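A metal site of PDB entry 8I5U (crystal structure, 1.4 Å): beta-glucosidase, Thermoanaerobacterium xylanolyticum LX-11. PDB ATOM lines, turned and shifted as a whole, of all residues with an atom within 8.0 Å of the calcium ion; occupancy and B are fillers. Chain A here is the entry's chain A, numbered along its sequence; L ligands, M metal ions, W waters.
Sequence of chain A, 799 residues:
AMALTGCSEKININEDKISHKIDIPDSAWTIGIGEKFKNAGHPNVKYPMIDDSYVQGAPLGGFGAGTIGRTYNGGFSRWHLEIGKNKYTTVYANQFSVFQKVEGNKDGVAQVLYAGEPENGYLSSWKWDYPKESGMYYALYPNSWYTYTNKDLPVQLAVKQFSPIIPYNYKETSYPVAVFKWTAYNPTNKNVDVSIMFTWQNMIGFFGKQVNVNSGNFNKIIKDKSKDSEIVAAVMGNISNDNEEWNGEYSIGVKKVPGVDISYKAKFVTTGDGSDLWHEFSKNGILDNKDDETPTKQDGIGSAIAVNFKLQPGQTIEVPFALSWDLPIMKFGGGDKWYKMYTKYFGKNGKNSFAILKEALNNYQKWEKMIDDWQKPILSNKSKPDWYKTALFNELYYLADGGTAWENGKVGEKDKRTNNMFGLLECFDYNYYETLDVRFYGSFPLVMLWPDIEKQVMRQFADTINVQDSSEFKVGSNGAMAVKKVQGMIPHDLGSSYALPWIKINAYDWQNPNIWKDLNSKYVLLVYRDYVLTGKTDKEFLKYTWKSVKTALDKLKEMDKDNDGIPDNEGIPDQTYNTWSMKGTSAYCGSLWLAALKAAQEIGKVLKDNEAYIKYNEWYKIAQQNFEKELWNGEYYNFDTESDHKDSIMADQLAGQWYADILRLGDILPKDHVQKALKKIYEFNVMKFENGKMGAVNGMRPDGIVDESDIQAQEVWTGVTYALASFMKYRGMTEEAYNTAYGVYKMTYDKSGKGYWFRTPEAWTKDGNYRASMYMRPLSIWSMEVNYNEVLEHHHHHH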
ATOM      1  N   LYS A 557       2.121 -14.009 -31.364  1.00  0.00           N
ATOM      2  CA  LYS A 557       3.576 -14.122 -31.598  1.00  0.00           C
ATOM      3  C   LYS A 557       4.383 -13.110 -30.778  1.00  0.00           C
ATOM      4  O   LYS A 557       5.491 -13.406 -30.343  1.00  0.00           O
ATOM      5  CB  LYS A 557       3.888 -13.961 -33.087  1.00  0.00           C
ATOM      6  CG  LYS A 557       5.349 -14.151 -33.491  1.00  0.00           C
ATOM      7  CD  LYS A 557       5.910 -15.493 -33.033  1.00  0.00           C
ATOM      8  CE  LYS A 557       7.017 -16.001 -33.929  1.00  0.00           C
ATOM      9  NZ  LYS A 557       8.207 -15.108 -33.994  1.00  0.00           N
ATOM     10  N   MET A 559       3.918 -12.230 -27.836  1.00  0.00           N
ATOM     11  CA  MET A 559       4.032 -12.695 -26.467  1.00  0.00           C
ATOM     12  C   MET A 559       5.126 -13.743 -26.264  1.00  0.00           C
ATOM     13  O   MET A 559       5.285 -14.262 -25.174  1.00  0.00           O
ATOM     14  CB  MET A 559       2.686 -13.223 -26.001  1.00  0.00           C
ATOM     15  CG  MET A 559       1.621 -12.144 -26.048  1.00  0.00           C
ATOM     16  SD  MET A 559       0.008 -12.827 -25.672  1.00  0.00           S
ATOM     17  CE  MET A 559      -0.991 -11.344 -25.613  1.00  0.00           C
ATOM     18  N   ASP A 560       5.872 -14.058 -27.323  1.00  0.00           N
ATOM     19  CA  ASP A 560       7.074 -14.884 -27.210  1.00  0.00           C
ATOM     20  C   ASP A 560       8.211 -14.005 -26.654  1.00  0.00           C
ATOM     21  O   ASP A 560       8.788 -13.234 -27.390  1.00  0.00           O
ATOM     22  CB  ASP A 560       7.439 -15.463 -28.573  1.00  0.00           C
ATOM     23  CG  ASP A 560       8.736 -16.259 -28.577  1.00  0.00           C
ATOM     24  OD1 ASP A 560       9.179 -16.693 -27.501  1.00  0.00           O
ATOM     25  OD2 ASP A 560       9.286 -16.453 -29.673  1.00  0.00           O
ATOM     26  N   LYS A 561       8.500 -14.150 -25.367  1.00  0.00           N
ATOM     27  CA  LYS A 561       9.521 -13.325 -24.677  1.00  0.00           C
ATOM     28  C   LYS A 561      10.965 -13.694 -25.014  1.00  0.00           C
ATOM     29  O   LYS A 561      11.839 -12.833 -25.027  1.00  0.00           O
ATOM     30  CB  LYS A 561       9.363 -13.420 -23.161  1.00  0.00           C
ATOM     31  CG  LYS A 561       8.079 -12.848 -22.597  1.00  0.00           C
ATOM     32  CD  LYS A 561       7.920 -13.261 -21.138  1.00  0.00           C
ATOM     33  CE  LYS A 561       6.838 -12.475 -20.421  1.00  0.00           C
ATOM     34  NZ  LYS A 561       6.669 -12.936 -19.016  1.00  0.00           N
ATOM     35  N   ASP A 562      11.213 -14.979 -25.267  1.00  0.00           N
ATOM     36  CA  ASP A 562      12.590 -15.506 -25.353  1.00  0.00           C
ATOM     37  C   ASP A 562      12.985 -16.020 -26.729  1.00  0.00           C
ATOM     38  O   ASP A 562      13.988 -16.739 -26.869  1.00  0.00           O
ATOM     39  CB  ASP A 562      12.761 -16.616 -24.314  1.00  0.00           C
ATOM     40  CG  ASP A 562      11.992 -17.872 -24.660  1.00  0.00           C
ATOM     41  OD1 ASP A 562      10.951 -17.779 -25.363  1.00  0.00           O
ATOM     42  OD2 ASP A 562      12.402 -18.967 -24.238  1.00  0.00           O
ATOM     43  N   ASN A 563      12.195 -15.681 -27.756  1.00  0.00           N
ATOM     44  CA  ASN A 563      12.485 -16.015 -29.140  1.00  0.00           C
ATOM     45  C   ASN A 563      12.635 -17.519 -29.451  1.00  0.00           C
ATOM     46  O   ASN A 563      13.377 -17.886 -30.365  1.00  0.00           O
ATOM     47  CB  ASN A 563      13.734 -15.235 -29.622  1.00  0.00           C
ATOM     48  CG  ASN A 563      13.835 -15.148 -31.131  1.00  0.00           C
ATOM     49  OD1 ASN A 563      12.823 -15.121 -31.845  1.00  0.00           O
ATOM     50  ND2 ASN A 563      15.067 -15.104 -31.638  1.00  0.00           N
ATOM     51  N   ASP A 564      11.917 -18.377 -28.715  1.00  0.00           N
ATOM     52  CA  ASP A 564      11.828 -19.793 -29.092  1.00  0.00           C
ATOM     53  C   ASP A 564      10.689 -20.073 -30.095  1.00  0.00           C
ATOM     54  O   ASP A 564      10.477 -21.209 -30.482  1.00  0.00           O
ATOM     55  CB  ASP A 564      11.725 -20.737 -27.874  1.00  0.00           C
ATOM     56  CG  ASP A 564      10.342 -20.767 -27.245  1.00  0.00           C
ATOM     57  OD1 ASP A 564       9.518 -19.866 -27.484  1.00  0.00           O
ATOM     58  OD2 ASP A 564      10.096 -21.686 -26.439  1.00  0.00           O
ATOM     59  N   GLY A 565       9.969 -19.025 -30.510  1.00  0.00           N
ATOM     60  CA  GLY A 565       8.921 -19.151 -31.526  1.00  0.00           C
ATOM     61  C   GLY A 565       7.536 -19.441 -30.943  1.00  0.00           C
ATOM     62  O   GLY A 565       6.584 -19.586 -31.701  1.00  0.00           O
ATOM     63  N   ILE A 566       7.431 -19.494 -29.624  1.00  0.00           N
ATOM     64  CA  ILE A 566       6.206 -19.925 -28.923  1.00  0.00           C
ATOM     65  C   ILE A 566       5.824 -18.846 -27.902  1.00  0.00           C
ATOM     66  O   ILE A 566       6.670 -18.370 -27.154  1.00  0.00           O
ATOM     67  CB  ILE A 566       6.423 -21.267 -28.199  1.00  0.00           C
ATOM     68  CG1 ILE A 566       6.962 -22.331 -29.167  1.00  0.00           C
ATOM     69  CG2 ILE A 566       5.130 -21.753 -27.545  1.00  0.00           C
ATOM     70  CD1 ILE A 566       7.415 -23.611 -28.507  1.00  0.00           C
ATOM     71  N   PRO A 567       4.544 -18.446 -27.853  1.00  0.00           N
ATOM     72  CA  PRO A 567       4.159 -17.513 -26.789  1.00  0.00           C
ATOM     73  C   PRO A 567       4.477 -18.048 -25.378  1.00  0.00           C
ATOM     74  O   PRO A 567       4.343 -19.245 -25.119  1.00  0.00           O
ATOM     75  CB  PRO A 567       2.639 -17.343 -26.992  1.00  0.00           C
ATOM     76  CG  PRO A 567       2.229 -18.510 -27.822  1.00  0.00           C
ATOM     77  CD  PRO A 567       3.392 -18.841 -28.690  1.00  0.00           C
ATOM     78  N   ASP A 568       4.917 -17.167 -24.477  1.00  0.00           N
ATOM     79  CA  ASP A 568       5.284 -17.571 -23.121  1.00  0.00           C
ATOM     80  C   ASP A 568       4.106 -17.428 -22.185  1.00  0.00           C
ATOM     81  O   ASP A 568       3.536 -16.333 -22.067  1.00  0.00           O
ATOM     82  CB  ASP A 568       6.413 -16.693 -22.558  1.00  0.00           C
ATOM     83  CG  ASP A 568       7.740 -16.982 -23.198  1.00  0.00           C
ATOM     84  OD1 ASP A 568       7.868 -16.782 -24.423  1.00  0.00           O
ATOM     85  OD2 ASP A 568       8.668 -17.422 -22.487  1.00  0.00           O
ATOM     86  N   ASN A 569       3.739 -18.504 -21.497  1.00  0.00           N
ATOM     87  CA  ASN A 569       2.854 -18.374 -20.348  1.00  0.00           C
ATOM     88  C   ASN A 569       3.600 -17.613 -19.242  1.00  0.00           C
ATOM     89  O   ASN A 569       4.809 -17.764 -19.097  1.00  0.00           O
ATOM     90  CB  ASN A 569       2.346 -19.734 -19.849  1.00  0.00           C
ATOM     91  CG  ASN A 569       1.429 -20.413 -20.844  1.00  0.00           C
ATOM     92  OD1 ASN A 569       1.853 -21.294 -21.607  1.00  0.00           O
ATOM     93  ND2 ASN A 569       0.161 -19.985 -20.870  1.00  0.00           N
ATOM     94  N   GLY A 584       6.416 -20.232 -19.076  1.00  0.00           N
ATOM     95  CA  GLY A 584       7.273 -20.601 -20.185  1.00  0.00           C
ATOM     96  C   GLY A 584       6.471 -21.215 -21.312  1.00  0.00           C
ATOM     97  O   GLY A 584       5.387 -20.733 -21.629  1.00  0.00           O
ATOM     98  N   THR A 585       7.003 -22.267 -21.915  1.00  0.00           N
ATOM     99  CA  THR A 585       6.274 -22.991 -22.945  1.00  0.00           C
ATOM    100  C   THR A 585       5.478 -24.078 -22.244  1.00  0.00           C
ATOM    101  O   THR A 585       6.043 -24.876 -21.516  1.00  0.00           O
ATOM    102  CB  THR A 585       7.230 -23.627 -23.975  1.00  0.00           C
ATOM    103  OG1 THR A 585       7.884 -22.586 -24.701  1.00  0.00           O
ATOM    104  CG2 THR A 585       6.477 -24.521 -24.944  1.00  0.00           C
ATOM    105  N   TRP A 593      -0.975 -23.519 -30.117  1.00  0.00           N
ATOM    106  CA  TRP A 593      -0.238 -22.616 -31.011  1.00  0.00           C
ATOM    107  C   TRP A 593       0.258 -23.319 -32.272  1.00  0.00           C
ATOM    108  O   TRP A 593       0.062 -22.844 -33.370  1.00  0.00           O
ATOM    109  CB  TRP A 593       0.926 -22.014 -30.226  1.00  0.00           C
ATOM    110  CG  TRP A 593       1.935 -21.190 -30.979  1.00  0.00           C
ATOM    111  CD1 TRP A 593       3.257 -21.477 -31.128  1.00  0.00           C
ATOM    112  CD2 TRP A 593       1.707 -19.944 -31.640  1.00  0.00           C
ATOM    113  NE1 TRP A 593       3.884 -20.480 -31.832  1.00  0.00           N
ATOM    114  CE2 TRP A 593       2.963 -19.514 -32.160  1.00  0.00           C
ATOM    115  CE3 TRP A 593       0.595 -19.131 -31.838  1.00  0.00           C
ATOM    116  CZ2 TRP A 593       3.098 -18.321 -32.883  1.00  0.00           C
ATOM    117  CZ3 TRP A 593       0.742 -17.929 -32.544  1.00  0.00           C
ATOM    118  CH2 TRP A 593       2.000 -17.539 -33.053  1.00  0.00           C
ATOM    119  N   ASN A 626      11.202 -26.566 -31.276  1.00  0.00           N
ATOM    120  CA  ASN A 626      11.469 -26.145 -29.906  1.00  0.00           C
ATOM    121  C   ASN A 626      10.472 -26.733 -28.911  1.00  0.00           C
ATOM    122  O   ASN A 626      10.868 -27.095 -27.797  1.00  0.00           O
ATOM    123  CB  ASN A 626      11.535 -24.620 -29.807  1.00  0.00           C
ATOM    124  CG  ASN A 626      12.785 -24.057 -30.480  1.00  0.00           C
ATOM    125  OD1 ASN A 626      13.822 -24.729 -30.520  1.00  0.00           O
ATOM    126  ND2 ASN A 626      12.697 -22.856 -30.996  1.00  0.00           N
ATOM    127  N   GLU A 630      11.861 -28.838 -25.803  1.00  0.00           N
ATOM    128  CA  GLU A 630      11.592 -28.305 -24.478  1.00  0.00           C
ATOM    129  C   GLU A 630      10.758 -29.228 -23.595  1.00  0.00           C
ATOM    130  O   GLU A 630      10.961 -29.237 -22.384  1.00  0.00           O
ATOM    131  CB  GLU A 630      10.871 -26.968 -24.589  1.00  0.00           C
ATOM    132  CG  GLU A 630      11.780 -25.844 -25.061  1.00  0.00           C
ATOM    133  CD  GLU A 630      11.004 -24.655 -25.562  1.00  0.00           C
ATOM    134  OE1 GLU A 630       9.803 -24.550 -25.224  1.00  0.00           O
ATOM    135  OE2 GLU A 630      11.575 -23.835 -26.295  1.00  0.00           O
ATOM    136  N   THR A 641       7.689 -25.526 -19.067  1.00  0.00           N
ATOM    137  CA  THR A 641       9.147 -25.456 -18.921  1.00  0.00           C
ATOM    138  C   THR A 641       9.641 -24.799 -17.636  1.00  0.00           C
ATOM    139  O   THR A 641      10.830 -24.969 -17.281  1.00  0.00           O
ATOM    140  CB  THR A 641       9.774 -24.705 -20.097  1.00  0.00           C
ATOM    141  OG1 THR A 641       9.188 -23.413 -20.212  1.00  0.00           O
ATOM    142  CG2 THR A 641       9.599 -25.477 -21.367  1.00  0.00           C
ATOM    143  N   GLU A 642       8.795 -24.054 -16.941  1.00  0.00           N
ATOM    144  CA  GLU A 642       9.258 -23.196 -15.827  1.00  0.00           C
ATOM    145  C   GLU A 642       8.525 -23.284 -14.489  1.00  0.00           C
ATOM    146  O   GLU A 642       8.960 -22.682 -13.514  1.00  0.00           O
ATOM    147  CB  GLU A 642       9.307 -21.740 -16.292  1.00  0.00           C
ATOM    148  CG  GLU A 642      10.319 -21.485 -17.409  1.00  0.00           C
ATOM    149  CD  GLU A 642      10.412 -20.028 -17.819  1.00  0.00           C
ATOM    150  OE1 GLU A 642      10.332 -19.146 -16.936  1.00  0.00           O
ATOM    151  OE2 GLU A 642      10.581 -19.764 -19.027  1.00  0.00           O
HETATM  152  C1  LIG L   1      11.466 -22.406 -23.111  1.00  0.00           C
HETATM  153  O1  LIG L   1      12.552 -23.204 -22.622  1.00  0.00           O
HETATM  154  C2  LIG L   1      11.247 -21.210 -22.185  1.00  0.00           C
HETATM  155  O2  LIG L   1      10.973 -21.677 -20.863  1.00  0.00           O
HETATM  156  C3  LIG L   1      10.091 -20.305 -22.592  1.00  0.00           C
HETATM  157  O3  LIG L   1       9.927 -20.125 -24.006  1.00  0.00           O
HETATM  158 CA    CA M   1       8.689 -18.360 -25.879  1.00  0.00          CA
HETATM  159  O   HOH W   1       7.422 -19.905 -24.674  1.00  0.00           O
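The calcium ion is bound by OD1 of Asp 568, water W1, OD1 of Asp 564, OD1 of Asp 560, O of Ile 566, OD1 of Asp 562 and O3 of the ligand. The calcium ion has seven donor atoms within binding distance.
Within 4 Å of the calcium ion: Asp 560, Asp 562, Asp 564, Ile 566 and Asp 568. The nearest printed residue that does not touch the calcium ion is Lys 561 (4.2 Å).
OD2 of Asp 564 sits close to OE2 of Glu 630. The side-chain carboxylate (OD2) of Asp 560 is in hydrogen-bond range of the backbone NH (N) of Gly 565 (2.8 Å). The side-chain carboxylate (OD2) of Asp 564 sits at hydrogen-bond distance from the side-chain hydroxyl (OG1) of Thr 585, 3.0 Å away. O of Asp 564 is in hydrogen-bond range of ND2 of Asn 626, at 2.8 Å. N of Asp 568 lies within hydrogen-bond range of O of Met 559 (3.0 Å). The side-chain carboxylate of Asp 560 sits close to the backbone NH of Asn 563 (3.2 Å). N of Lys 561 lies close to OD1 of Asp 568.
Water W1 lies within hydrogen-bond range of the side-chain hydroxyl (OG1) of Thr 585 (2.7 Å) and the backbone carbonyl oxygen (O) of Pro 567 (3.2 Å).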
